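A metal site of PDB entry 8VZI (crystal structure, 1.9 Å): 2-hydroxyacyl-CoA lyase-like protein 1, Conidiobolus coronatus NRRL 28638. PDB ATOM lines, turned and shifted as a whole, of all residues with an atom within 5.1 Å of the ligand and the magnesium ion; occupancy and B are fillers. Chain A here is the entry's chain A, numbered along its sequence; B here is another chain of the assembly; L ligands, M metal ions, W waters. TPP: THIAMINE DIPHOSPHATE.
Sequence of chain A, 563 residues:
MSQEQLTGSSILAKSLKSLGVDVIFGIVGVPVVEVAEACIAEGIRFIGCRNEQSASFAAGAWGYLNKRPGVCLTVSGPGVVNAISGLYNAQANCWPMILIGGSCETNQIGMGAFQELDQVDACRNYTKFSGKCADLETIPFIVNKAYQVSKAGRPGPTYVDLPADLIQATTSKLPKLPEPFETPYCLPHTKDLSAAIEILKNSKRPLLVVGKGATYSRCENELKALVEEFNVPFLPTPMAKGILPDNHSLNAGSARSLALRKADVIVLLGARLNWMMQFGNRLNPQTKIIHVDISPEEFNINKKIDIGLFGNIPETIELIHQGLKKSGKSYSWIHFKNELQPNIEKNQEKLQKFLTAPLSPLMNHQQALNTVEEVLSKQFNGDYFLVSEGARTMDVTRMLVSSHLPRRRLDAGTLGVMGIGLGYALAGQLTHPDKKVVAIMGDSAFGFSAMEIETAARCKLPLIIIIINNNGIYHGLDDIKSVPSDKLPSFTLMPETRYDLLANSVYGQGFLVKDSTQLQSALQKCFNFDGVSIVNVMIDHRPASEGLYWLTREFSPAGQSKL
Of the 31 residues printed, 3 come within 4 Å of the magnesium ion.
Along chain A the residues within 4 Å of the magnesium ion span positions 443 to 472.
The nearest printed residue that does not touch the magnesium ion is Ser 444 (4.2 Å).
The backbone NH of Asp 443 sits at hydrogen-bond distance from the backbone carbonyl oxygen of Ile 468.
OD2 of Asp 443 lies within hydrogen-bond range of N of Asn 471 (3.3 Å).
ND2 of Asn 82 of chain B is in hydrogen-bond range of OE1 of Glu 52 of chain B (3.0 Å).
NH1 of Arg 392 is in hydrogen-bond range of O of Tyr 474 (2.9 Å).
The backbone carbonyl oxygen (O) of Gly 416 sits at hydrogen-bond distance from the side-chain amide nitrogen (NE2) of Gln 115 of chain B, at 3.4 Å.
N of Gly 390 is in hydrogen-bond range of SD of Met 418, 3.6 Å away.
The backbone NH of Gly 442 is in hydrogen-bond range of the backbone carbonyl oxygen of Glu 389 (3.0 Å).
O of Pro 78 of chain B sits close to OD1 of Asn 82 of chain B (3.5 Å).
The magnesium ion is bound by an oxygen (O2A) of the ligand (2.0 Å), the side-chain amide oxygen of Asn 470 (2.1 Å), the side-chain carboxylate of Asp 443 (2.1 Å), water W3 (2.2 Å), an oxygen (O1B) of the ligand (2.2 Å) and the backbone carbonyl oxygen of Gly 472 (2.2 Å).
The magnesium ion has six donor atoms within binding distance.
Water W3 lies within hydrogen-bond range of the backbone carbonyl oxygen (O) of Ile 468 (2.6 Å), an oxygen (O2B) of the ligand (2.8 Å) and the side-chain hydroxyl (OG1) of Thr 393 (3.5 Å).
Water W1 lies within hydrogen-bond range of a nitrogen (N4') of the ligand and the side-chain amide nitrogen of Gln 115 of chain B.
Water W2 bridges the side-chain hydroxyl of Tyr 474 (2.7 Å) and the backbone NH of Val 30 of chain B (2.9 Å).
Gly 390 touches the ligand.
CA of Gly 442 touches O1A of the ligand, at 3.3 Å.
CZ of Phe 448 touches N1' of the ligand, at 3.5 Å.
CA of Ile 473 touches O7 of the ligand, at 3.5 Å.
Ile 27 of chain B touches the ligand (CG2 to CM4, 3.8 Å).
Val 28 of chain B touches the ligand.
CA of Gly 29 of chain B touches C7' of the ligand, at 3.99 Å.
Val 75 of chain B touches the ligand (CG2 to C6', 3.7 Å).
ND2 of Asn 82 of chain B touches CM2 of the ligand, at 3.6 Å.
Gln 115 of chain B touches the ligand (NE2 to N4', 3.5 Å).
Hydrophobic or aromatic side chains within 4 Å of the ligand: His 365, Ala 391, Met 418, Ala 445, Phe 448, Ile 473, Ile 27 of chain B and Val 75 of chain B.
23 residues have an atom within 4 Å of the ligand: His 365, Gly 390, Ala 391, Arg 392, Thr 393, Gly 416, Met 418, Gly 442, Asp 443, Ser 444, Ala 445, Phe 448, Asn 470, Gly 472, Ile 473, Tyr 474, Ile 27 of chain B, Val 28 of chain B, Gly 29 of chain B, Glu 52 of chain B, Val 75 of chain B, Asn 82 of chain B and Gln 115 of chain B.
The nearest printed residue that does not touch the ligand is Pro 78 of chain B (4.1 Å).
An oxygen (O2A) of the ligand lies close to the backbone NH (N) of Asp 443.
OE2 of Glu 52 of chain B lies within hydrogen-bond range of N1' of the ligand (2.6 Å).
The backbone NH of Thr 393 lies within hydrogen-bond range of an oxygen (O2B) of the ligand, 3.0 Å away.
O2B of the ligand lies within hydrogen-bond range of OG1 of Thr 393, 2.6 Å away.
N of Arg 392 sits at hydrogen-bond distance from O3B of the ligand, at 2.7 Å.
O of Gly 416 sits at hydrogen-bond distance from N4' of the ligand (2.8 Å).
A ring nitrogen (NE2) of His 365 is in hydrogen-bond range of an oxygen (O2B) of the ligand.
The backbone NH of Ser 444 lies close to an oxygen (O2A) of the ligand (3.0 Å).
The backbone NH (N) of Ala 445 lies within hydrogen-bond range of an oxygen (O1A) of the ligand (3.0 Å).
An oxygen (O3B) of the ligand lies close to the backbone NH of Tyr 474 (3.5 Å).
O3A of the ligand lies within hydrogen-bond range of N of Ala 391 (3.4 Å).
The backbone NH (N) of Met 418 lies within hydrogen-bond range of a nitrogen (N3') of the ligand, at 3.2 Å.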
ATOM      1  N   HIS A 365     -18.419 -20.456  10.416  1.00  0.00           N
ATOM      2  CA  HIS A 365     -17.153 -21.056  10.012  1.00  0.00           C
ATOM      3  C   HIS A 365     -16.044 -20.778  11.041  1.00  0.00           C
ATOM      4  O   HIS A 365     -15.332 -21.689  11.469  1.00  0.00           O
ATOM      5  CB  HIS A 365     -16.716 -20.526   8.651  1.00  0.00           C
ATOM      6  CG  HIS A 365     -17.471 -21.082   7.477  1.00  0.00           C
ATOM      7  ND1 HIS A 365     -18.638 -20.527   7.011  1.00  0.00           N
ATOM      8  CD2 HIS A 365     -17.168 -22.083   6.621  1.00  0.00           C
ATOM      9  CE1 HIS A 365     -19.048 -21.180   5.940  1.00  0.00           C
ATOM     10  NE2 HIS A 365     -18.170 -22.134   5.678  1.00  0.00           N
ATOM     11  N   GLU A 389      -9.534 -28.225   2.330  1.00  0.00           N
ATOM     12  CA  GLU A 389     -10.174 -28.132   1.028  1.00  0.00           C
ATOM     13  C   GLU A 389     -11.601 -27.624   1.179  1.00  0.00           C
ATOM     14  O   GLU A 389     -12.321 -28.038   2.080  1.00  0.00           O
ATOM     15  CB  GLU A 389     -10.172 -29.496   0.342  1.00  0.00           C
ATOM     16  CG  GLU A 389     -10.874 -29.562  -0.968  1.00  0.00           C
ATOM     17  CD  GLU A 389     -10.999 -30.992  -1.453  1.00  0.00           C
ATOM     18  OE1 GLU A 389     -11.413 -31.864  -0.658  1.00  0.00           O
ATOM     19  OE2 GLU A 389     -10.646 -31.258  -2.613  1.00  0.00           O
ATOM     20  N   GLY A 390     -12.008 -26.749   0.278  1.00  0.00           N
ATOM     21  CA  GLY A 390     -13.295 -26.104   0.352  1.00  0.00           C
ATOM     22  C   GLY A 390     -13.164 -24.703  -0.183  1.00  0.00           C
ATOM     23  O   GLY A 390     -12.137 -24.337  -0.755  1.00  0.00           O
ATOM     24  N   ALA A 391     -14.215 -23.908   0.007  1.00  0.00           N
ATOM     25  CA  ALA A 391     -14.134 -22.493  -0.337  1.00  0.00           C
ATOM     26  C   ALA A 391     -14.009 -21.669   0.933  1.00  0.00           C
ATOM     27  O   ALA A 391     -12.898 -21.342   1.359  1.00  0.00           O
ATOM     28  CB  ALA A 391     -15.341 -22.063  -1.171  1.00  0.00           C
ATOM     29  N   ARG A 392     -15.129 -21.347   1.585  1.00  0.00           N
ATOM     30  CA  ARG A 392     -15.032 -20.601   2.831  1.00  0.00           C
ATOM     31  C   ARG A 392     -14.357 -21.427   3.918  1.00  0.00           C
ATOM     32  O   ARG A 392     -13.558 -20.902   4.707  1.00  0.00           O
ATOM     33  CB  ARG A 392     -16.410 -20.108   3.259  1.00  0.00           C
ATOM     34  CG  ARG A 392     -17.017 -19.157   2.227  1.00  0.00           C
ATOM     35  CD  ARG A 392     -18.449 -18.793   2.590  1.00  0.00           C
ATOM     36  NE  ARG A 392     -18.528 -18.084   3.863  1.00  0.00           N
ATOM     37  CZ  ARG A 392     -19.644 -17.906   4.536  1.00  0.00           C
ATOM     38  NH1 ARG A 392     -20.795 -18.395   4.113  1.00  0.00           N
ATOM     39  NH2 ARG A 392     -19.613 -17.222   5.675  1.00  0.00           N
ATOM     40  N   THR A 393     -14.642 -22.740   3.962  1.00  0.00           N
ATOM     41  CA  THR A 393     -13.947 -23.610   4.913  1.00  0.00           C
ATOM     42  C   THR A 393     -12.433 -23.527   4.746  1.00  0.00           C
ATOM     43  O   THR A 393     -11.695 -23.446   5.738  1.00  0.00           O
ATOM     44  CB  THR A 393     -14.439 -25.050   4.744  1.00  0.00           C
ATOM     45  OG1 THR A 393     -15.831 -25.130   5.097  1.00  0.00           O
ATOM     46  CG2 THR A 393     -13.655 -25.967   5.677  1.00  0.00           C
ATOM     47  N   GLY A 416      -7.003 -24.502  -7.381  1.00  0.00           N
ATOM     48  CA  GLY A 416      -8.212 -24.412  -6.579  1.00  0.00           C
ATOM     49  C   GLY A 416      -9.147 -25.571  -6.813  1.00  0.00           C
ATOM     50  O   GLY A 416     -10.370 -25.373  -6.940  1.00  0.00           O
ATOM     51  N   VAL A 417      -8.605 -26.783  -6.903  1.00  0.00           N
ATOM     52  CA  VAL A 417      -9.378 -27.953  -7.284  1.00  0.00           C
ATOM     53  C   VAL A 417     -10.049 -28.555  -6.049  1.00  0.00           C
ATOM     54  O   VAL A 417      -9.395 -28.802  -5.023  1.00  0.00           O
ATOM     55  CB  VAL A 417      -8.481 -28.990  -7.972  1.00  0.00           C
ATOM     56  CG1 VAL A 417      -7.198 -29.192  -7.199  1.00  0.00           C
ATOM     57  CG2 VAL A 417      -9.223 -30.310  -8.149  1.00  0.00           C
ATOM     58  N   MET A 418     -11.361 -28.775  -6.145  1.00  0.00           N
ATOM     59  CA  MET A 418     -12.043 -29.610  -5.159  1.00  0.00           C
ATOM     60  C   MET A 418     -11.911 -31.074  -5.571  1.00  0.00           C
ATOM     61  O   MET A 418     -11.925 -31.405  -6.748  1.00  0.00           O
ATOM     62  CB  MET A 418     -13.523 -29.242  -5.054  1.00  0.00           C
ATOM     63  CG  MET A 418     -13.806 -27.800  -4.671  1.00  0.00           C
ATOM     64  SD  MET A 418     -13.212 -27.385  -3.026  1.00  0.00           S
ATOM     65  CE  MET A 418     -11.665 -26.561  -3.407  1.00  0.00           C
ATOM     66  N   GLY A 442     -14.861 -28.787   3.396  1.00  0.00           N
ATOM     67  CA  GLY A 442     -16.240 -28.390   3.220  1.00  0.00           C
ATOM     68  C   GLY A 442     -17.109 -29.557   2.809  1.00  0.00           C
ATOM     69  O   GLY A 442     -16.639 -30.559   2.275  1.00  0.00           O
ATOM     70  N   ASP A 443     -18.423 -29.429   3.078  1.00  0.00           N
ATOM     71  CA  ASP A 443     -19.327 -30.520   2.745  1.00  0.00           C
ATOM     72  C   ASP A 443     -19.381 -30.760   1.242  1.00  0.00           C
ATOM     73  O   ASP A 443     -19.368 -31.910   0.792  1.00  0.00           O
ATOM     74  CB  ASP A 443     -20.742 -30.280   3.325  1.00  0.00           C
ATOM     75  CG  ASP A 443     -21.377 -28.960   2.893  1.00  0.00           C
ATOM     76  OD1 ASP A 443     -20.729 -27.908   3.011  1.00  0.00           O
ATOM     77  OD2 ASP A 443     -22.551 -28.984   2.454  1.00  0.00           O
ATOM     78  N   SER A 444     -19.382 -29.688   0.433  1.00  0.00           N
ATOM     79  CA  SER A 444     -19.327 -29.895  -1.014  1.00  0.00           C
ATOM     80  C   SER A 444     -18.014 -30.551  -1.421  1.00  0.00           C
ATOM     81  O   SER A 444     -18.008 -31.556  -2.145  1.00  0.00           O
ATOM     82  CB  SER A 444     -19.528 -28.568  -1.756  1.00  0.00           C
ATOM     83  OG  SER A 444     -19.232 -28.716  -3.148  1.00  0.00           O
ATOM     84  N   ALA A 445     -16.893 -30.014  -0.943  1.00  0.00           N
ATOM     85  CA  ALA A 445     -15.589 -30.569  -1.295  1.00  0.00           C
ATOM     86  C   ALA A 445     -15.514 -32.055  -0.975  1.00  0.00           C
ATOM     87  O   ALA A 445     -15.009 -32.860  -1.772  1.00  0.00           O
ATOM     88  CB  ALA A 445     -14.485 -29.812  -0.564  1.00  0.00           C
ATOM     89  N   PHE A 448     -16.699 -34.916  -3.413  1.00  0.00           N
ATOM     90  CA  PHE A 448     -15.940 -35.293  -4.598  1.00  0.00           C
ATOM     91  C   PHE A 448     -15.183 -36.602  -4.396  1.00  0.00           C
ATOM     92  O   PHE A 448     -15.041 -37.381  -5.337  1.00  0.00           O
ATOM     93  CB  PHE A 448     -14.958 -34.183  -4.986  1.00  0.00           C
ATOM     94  CG  PHE A 448     -15.599 -33.006  -5.673  1.00  0.00           C
ATOM     95  CD1 PHE A 448     -16.228 -32.019  -4.934  1.00  0.00           C
ATOM     96  CD2 PHE A 448     -15.550 -32.890  -7.063  1.00  0.00           C
ATOM     97  CE1 PHE A 448     -16.807 -30.929  -5.567  1.00  0.00           C
ATOM     98  CE2 PHE A 448     -16.115 -31.804  -7.705  1.00  0.00           C
ATOM     99  CZ  PHE A 448     -16.746 -30.819  -6.956  1.00  0.00           C
ATOM    100  N   ILE A 468     -16.952 -29.323   7.623  1.00  0.00           N
ATOM    101  CA  ILE A 468     -17.647 -28.085   7.965  1.00  0.00           C
ATOM    102  C   ILE A 468     -18.835 -27.988   7.024  1.00  0.00           C
ATOM    103  O   ILE A 468     -18.673 -27.774   5.822  1.00  0.00           O
ATOM    104  CB  ILE A 468     -16.721 -26.871   7.841  1.00  0.00           C
ATOM    105  CG1 ILE A 468     -15.432 -27.096   8.641  1.00  0.00           C
ATOM    106  CG2 ILE A 468     -17.430 -25.595   8.298  1.00  0.00           C
ATOM    107  CD1 ILE A 468     -15.649 -27.236  10.183  1.00  0.00           C
ATOM    108  N   ASN A 470     -22.339 -26.562   5.784  1.00  0.00           N
ATOM    109  CA  ASN A 470     -23.330 -25.492   5.695  1.00  0.00           C
ATOM    110  C   ASN A 470     -24.404 -25.797   4.656  1.00  0.00           C
ATOM    111  O   ASN A 470     -25.089 -24.882   4.190  1.00  0.00           O
ATOM    112  CB  ASN A 470     -22.673 -24.152   5.399  1.00  0.00           C
ATOM    113  CG  ASN A 470     -21.895 -24.145   4.088  1.00  0.00           C
ATOM    114  OD1 ASN A 470     -21.736 -25.177   3.446  1.00  0.00           O
ATOM    115  ND2 ASN A 470     -21.384 -22.974   3.722  1.00  0.00           N
ATOM    116  N   ASN A 471     -24.562 -27.065   4.283  1.00  0.00           N
ATOM    117  CA  ASN A 471     -25.597 -27.495   3.342  1.00  0.00           C
ATOM    118  C   ASN A 471     -25.371 -26.924   1.945  1.00  0.00           C
ATOM    119  O   ASN A 471     -26.342 -26.654   1.234  1.00  0.00           O
ATOM    120  CB  ASN A 471     -27.011 -27.111   3.801  1.00  0.00           C
ATOM    121  CG  ASN A 471     -27.341 -27.639   5.183  1.00  0.00           C
ATOM    122  OD1 ASN A 471     -26.785 -28.633   5.634  1.00  0.00           O
ATOM    123  ND2 ASN A 471     -28.264 -26.964   5.846  1.00  0.00           N
ATOM    124  N   GLY A 472     -24.131 -26.718   1.513  1.00  0.00           N
ATOM    125  CA  GLY A 472     -23.971 -26.376   0.117  1.00  0.00           C
ATOM    126  C   GLY A 472     -22.617 -25.745  -0.190  1.00  0.00           C
ATOM    127  O   GLY A 472     -21.653 -25.891   0.568  1.00  0.00           O
ATOM    128  N   ILE A 473     -22.594 -25.039  -1.314  1.00  0.00           N
ATOM    129  CA  ILE A 473     -21.395 -24.471  -1.921  1.00  0.00           C
ATOM    130  C   ILE A 473     -21.344 -22.988  -1.528  1.00  0.00           C
ATOM    131  O   ILE A 473     -22.105 -22.178  -2.057  1.00  0.00           O
ATOM    132  CB  ILE A 473     -21.417 -24.650  -3.442  1.00  0.00           C
ATOM    133  CG1 ILE A 473     -21.574 -26.129  -3.796  1.00  0.00           C
ATOM    134  CG2 ILE A 473     -20.165 -24.051  -4.110  1.00  0.00           C
ATOM    135  CD1 ILE A 473     -21.899 -26.375  -5.246  1.00  0.00           C
ATOM    136  N   TYR A 474     -20.459 -22.649  -0.575  1.00  0.00           N
ATOM    137  CA  TYR A 474     -20.367 -21.326   0.054  1.00  0.00           C
ATOM    138  C   TYR A 474     -21.488 -21.083   1.050  1.00  0.00           C
ATOM    139  O   TYR A 474     -21.294 -20.423   2.070  1.00  0.00           O
ATOM    140  CB  TYR A 474     -20.365 -20.197  -0.991  1.00  0.00           C
ATOM    141  CG  TYR A 474     -19.114 -20.089  -1.831  1.00  0.00           C
ATOM    142  CD1 TYR A 474     -18.858 -20.996  -2.851  1.00  0.00           C
ATOM    143  CD2 TYR A 474     -18.197 -19.057  -1.617  1.00  0.00           C
ATOM    144  CE1 TYR A 474     -17.706 -20.883  -3.640  1.00  0.00           C
ATOM    145  CE2 TYR A 474     -17.060 -18.939  -2.397  1.00  0.00           C
ATOM    146  CZ  TYR A 474     -16.814 -19.852  -3.409  1.00  0.00           C
ATOM    147  OH  TYR A 474     -15.673 -19.723  -4.177  1.00  0.00           O
ATOM    148  N   HIS A 475     -22.683 -21.593   0.752  1.00  0.00           N
ATOM    149  CA  HIS A 475     -23.847 -21.455   1.617  1.00  0.00           C
ATOM    150  C   HIS A 475     -24.883 -22.473   1.159  1.00  0.00           C
ATOM    151  O   HIS A 475     -24.703 -23.162   0.153  1.00  0.00           O
ATOM    152  CB  HIS A 475     -24.421 -20.026   1.593  1.00  0.00           C
ATOM    153  CG  HIS A 475     -24.913 -19.597   0.243  1.00  0.00           C
ATOM    154  ND1 HIS A 475     -26.135 -18.995   0.043  1.00  0.00           N
ATOM    155  CD2 HIS A 475     -24.319 -19.660  -0.974  1.00  0.00           C
ATOM    156  CE1 HIS A 475     -26.286 -18.715  -1.243  1.00  0.00           C
ATOM    157  NE2 HIS A 475     -25.198 -19.120  -1.880  1.00  0.00           N
ATOM    158  N   ILE B  27     -21.993 -28.838 -11.637  1.00  0.00           N
ATOM    159  CA  ILE B  27     -21.540 -28.377 -10.325  1.00  0.00           C
ATOM    160  C   ILE B  27     -21.071 -26.937 -10.484  1.00  0.00           C
ATOM    161  O   ILE B  27     -20.322 -26.628 -11.418  1.00  0.00           O
ATOM    162  CB  ILE B  27     -20.413 -29.257  -9.758  1.00  0.00           C
ATOM    163  CG1 ILE B  27     -20.847 -30.715  -9.700  1.00  0.00           C
ATOM    164  CG2 ILE B  27     -19.994 -28.755  -8.352  1.00  0.00           C
ATOM    165  CD1 ILE B  27     -19.855 -31.620  -9.048  1.00  0.00           C
ATOM    166  N   VAL B  28     -21.505 -26.054  -9.588  1.00  0.00           N
ATOM    167  CA  VAL B  28     -21.313 -24.628  -9.767  1.00  0.00           C
ATOM    168  C   VAL B  28     -20.124 -24.150  -8.945  1.00  0.00           C
ATOM    169  O   VAL B  28     -19.552 -24.885  -8.140  1.00  0.00           O
ATOM    170  CB  VAL B  28     -22.580 -23.824  -9.425  1.00  0.00           C
ATOM    171  CG1 VAL B  28     -23.723 -24.251 -10.326  1.00  0.00           C
ATOM    172  CG2 VAL B  28     -22.938 -23.979  -7.930  1.00  0.00           C
ATOM    173  N   GLY B  29     -19.760 -22.887  -9.130  1.00  0.00           N
ATOM    174  CA  GLY B  29     -18.634 -22.272  -8.427  1.00  0.00           C
ATOM    175  C   GLY B  29     -18.291 -20.941  -9.062  1.00  0.00           C
ATOM    176  O   GLY B  29     -19.157 -20.245  -9.588  1.00  0.00           O
ATOM    177  N   VAL B  30     -16.994 -20.632  -9.046  1.00  0.00           N
ATOM    178  CA  VAL B  30     -16.453 -19.605  -9.948  1.00  0.00           C
ATOM    179  C   VAL B  30     -16.239 -20.232 -11.317  1.00  0.00           C
ATOM    180  O   VAL B  30     -15.658 -21.326 -11.417  1.00  0.00           O
ATOM    181  CB  VAL B  30     -15.144 -19.046  -9.397  1.00  0.00           C
ATOM    182  CG1 VAL B  30     -14.349 -18.346 -10.503  1.00  0.00           C
ATOM    183  CG2 VAL B  30     -15.424 -18.087  -8.230  1.00  0.00           C
ATOM    184  N   GLU B  52     -18.034 -33.999 -11.319  1.00  0.00           N
ATOM    185  CA  GLU B  52     -18.391 -33.737 -12.710  1.00  0.00           C
ATOM    186  C   GLU B  52     -18.385 -34.993 -13.572  1.00  0.00           C
ATOM    187  O   GLU B  52     -19.076 -35.016 -14.601  1.00  0.00           O
ATOM    188  CB  GLU B  52     -17.471 -32.697 -13.337  1.00  0.00           C
ATOM    189  CG  GLU B  52     -17.636 -31.298 -12.755  1.00  0.00           C
ATOM    190  CD  GLU B  52     -16.757 -31.079 -11.515  1.00  0.00           C
ATOM    191  OE1 GLU B  52     -16.051 -32.023 -11.102  1.00  0.00           O
ATOM    192  OE2 GLU B  52     -16.785 -29.954 -10.979  1.00  0.00           O
ATOM    193  N   VAL B  75     -17.340 -25.705 -13.923  1.00  0.00           N
ATOM    194  CA  VAL B  75     -16.447 -24.561 -13.725  1.00  0.00           C
ATOM    195  C   VAL B  75     -15.228 -24.715 -14.618  1.00  0.00           C
ATOM    196  O   VAL B  75     -14.998 -25.776 -15.215  1.00  0.00           O
ATOM    197  CB  VAL B  75     -16.031 -24.409 -12.248  1.00  0.00           C
ATOM    198  CG1 VAL B  75     -17.256 -24.445 -11.354  1.00  0.00           C
ATOM    199  CG2 VAL B  75     -15.013 -25.475 -11.862  1.00  0.00           C
ATOM    200  N   PRO B  78     -10.203 -27.519 -13.675  1.00  0.00           N
ATOM    201  CA  PRO B  78     -10.453 -28.907 -13.252  1.00  0.00           C
ATOM    202  C   PRO B  78     -11.917 -29.325 -13.372  1.00  0.00           C
ATOM    203  O   PRO B  78     -12.186 -30.532 -13.433  1.00  0.00           O
ATOM    204  CB  PRO B  78      -9.999 -28.913 -11.784  1.00  0.00           C
ATOM    205  CG  PRO B  78     -10.197 -27.517 -11.328  1.00  0.00           C
ATOM    206  CD  PRO B  78      -9.905 -26.636 -12.541  1.00  0.00           C
ATOM    207  N   GLY B  79     -12.862 -28.383 -13.404  1.00  0.00           N
ATOM    208  CA  GLY B  79     -14.243 -28.761 -13.662  1.00  0.00           C
ATOM    209  C   GLY B  79     -14.422 -29.366 -15.048  1.00  0.00           C
ATOM    210  O   GLY B  79     -14.995 -30.446 -15.213  1.00  0.00           O
ATOM    211  N   ASN B  82     -12.437 -32.839 -15.308  1.00  0.00           N
ATOM    212  CA  ASN B  82     -13.224 -33.935 -14.736  1.00  0.00           C
ATOM    213  C   ASN B  82     -14.327 -34.404 -15.700  1.00  0.00           C
ATOM    214  O   ASN B  82     -14.617 -35.607 -15.782  1.00  0.00           O
ATOM    215  CB  ASN B  82     -13.851 -33.513 -13.398  1.00  0.00           C
ATOM    216  CG  ASN B  82     -12.864 -33.532 -12.253  1.00  0.00           C
ATOM    217  OD1 ASN B  82     -11.691 -33.821 -12.448  1.00  0.00           O
ATOM    218  ND2 ASN B  82     -13.354 -33.224 -11.040  1.00  0.00           N
ATOM    219  N   GLN B 115      -7.485 -21.202 -12.660  1.00  0.00           N
ATOM    220  CA  GLN B 115      -8.041 -22.313 -13.437  1.00  0.00           C
ATOM    221  C   GLN B 115      -7.885 -22.049 -14.937  1.00  0.00           C
ATOM    222  O   GLN B 115      -8.770 -22.371 -15.735  1.00  0.00           O
ATOM    223  CB  GLN B 115      -9.509 -22.583 -13.059  1.00  0.00           C
ATOM    224  CG  GLN B 115      -9.637 -22.889 -11.552  1.00  0.00           C
ATOM    225  CD  GLN B 115     -11.015 -23.348 -11.090  1.00  0.00           C
ATOM    226  OE1 GLN B 115     -12.020 -23.058 -11.710  1.00  0.00           O
ATOM    227  NE2 GLN B 115     -11.048 -24.059  -9.958  1.00  0.00           N
HETATM  228  N1' TPP L   1     -15.341 -28.585  -9.311  1.00  0.00           N
HETATM  229  C2' TPP L   1     -14.010 -28.676  -9.116  1.00  0.00           C
HETATM  230  CM2 TPP L   1     -13.345 -29.927  -9.574  1.00  0.00           C
HETATM  231  N3' TPP L   1     -13.251 -27.751  -8.537  1.00  0.00           N
HETATM  232  C4' TPP L   1     -13.851 -26.609  -8.118  1.00  0.00           C
HETATM  233  N4' TPP L   1     -13.076 -25.685  -7.569  1.00  0.00           N
HETATM  234  C5' TPP L   1     -15.253 -26.409  -8.305  1.00  0.00           C
HETATM  235  C6' TPP L   1     -15.923 -27.456  -8.902  1.00  0.00           C
HETATM  236  C7' TPP L   1     -15.986 -25.190  -7.817  1.00  0.00           C
HETATM  237  N3  TPP L   1     -15.920 -25.042  -6.346  1.00  0.00           N
HETATM  238  C2  TPP L   1     -15.078 -24.228  -5.715  1.00  0.00           C
HETATM  239  S1  TPP L   1     -15.232 -24.308  -4.046  1.00  0.00           S
HETATM  240  C5  TPP L   1     -16.483 -25.487  -4.184  1.00  0.00           C
HETATM  241  C4  TPP L   1     -16.739 -25.772  -5.480  1.00  0.00           C
HETATM  242  CM4 TPP L   1     -17.740 -26.746  -5.999  1.00  0.00           C
HETATM  243  C6  TPP L   1     -17.147 -26.053  -2.953  1.00  0.00           C
HETATM  244  C7  TPP L   1     -17.403 -25.005  -1.903  1.00  0.00           C
HETATM  245  O7  TPP L   1     -18.210 -25.605  -0.854  1.00  0.00           O
HETATM  246  PA  TPP L   1     -17.618 -26.292   0.438  1.00  0.00           P
HETATM  247  O1A TPP L   1     -16.564 -27.285   0.148  1.00  0.00           O
HETATM  248  O2A TPP L   1     -18.851 -26.860   1.112  1.00  0.00           O
HETATM  249  O3A TPP L   1     -17.202 -25.014   1.225  1.00  0.00           O
HETATM  250  PB  TPP L   1     -17.905 -23.791   1.920  1.00  0.00           P
HETATM  251  O1B TPP L   1     -19.383 -24.024   1.866  1.00  0.00           O
HETATM  252  O2B TPP L   1     -17.336 -23.812   3.397  1.00  0.00           O
HETATM  253  O3B TPP L   1     -17.464 -22.593   1.174  1.00  0.00           O
HETATM  254 MG    MG M   1     -20.223 -25.975   2.268  1.00  0.00          MG
HETATM  255  O   HOH W   1     -13.348 -22.769  -7.996  1.00  0.00           O
HETATM  256  O   HOH W   2     -15.861 -21.195  -6.421  1.00  0.00           O
HETATM  257  O   HOH W   3     -19.059 -25.892   4.075  1.00  0.00           O
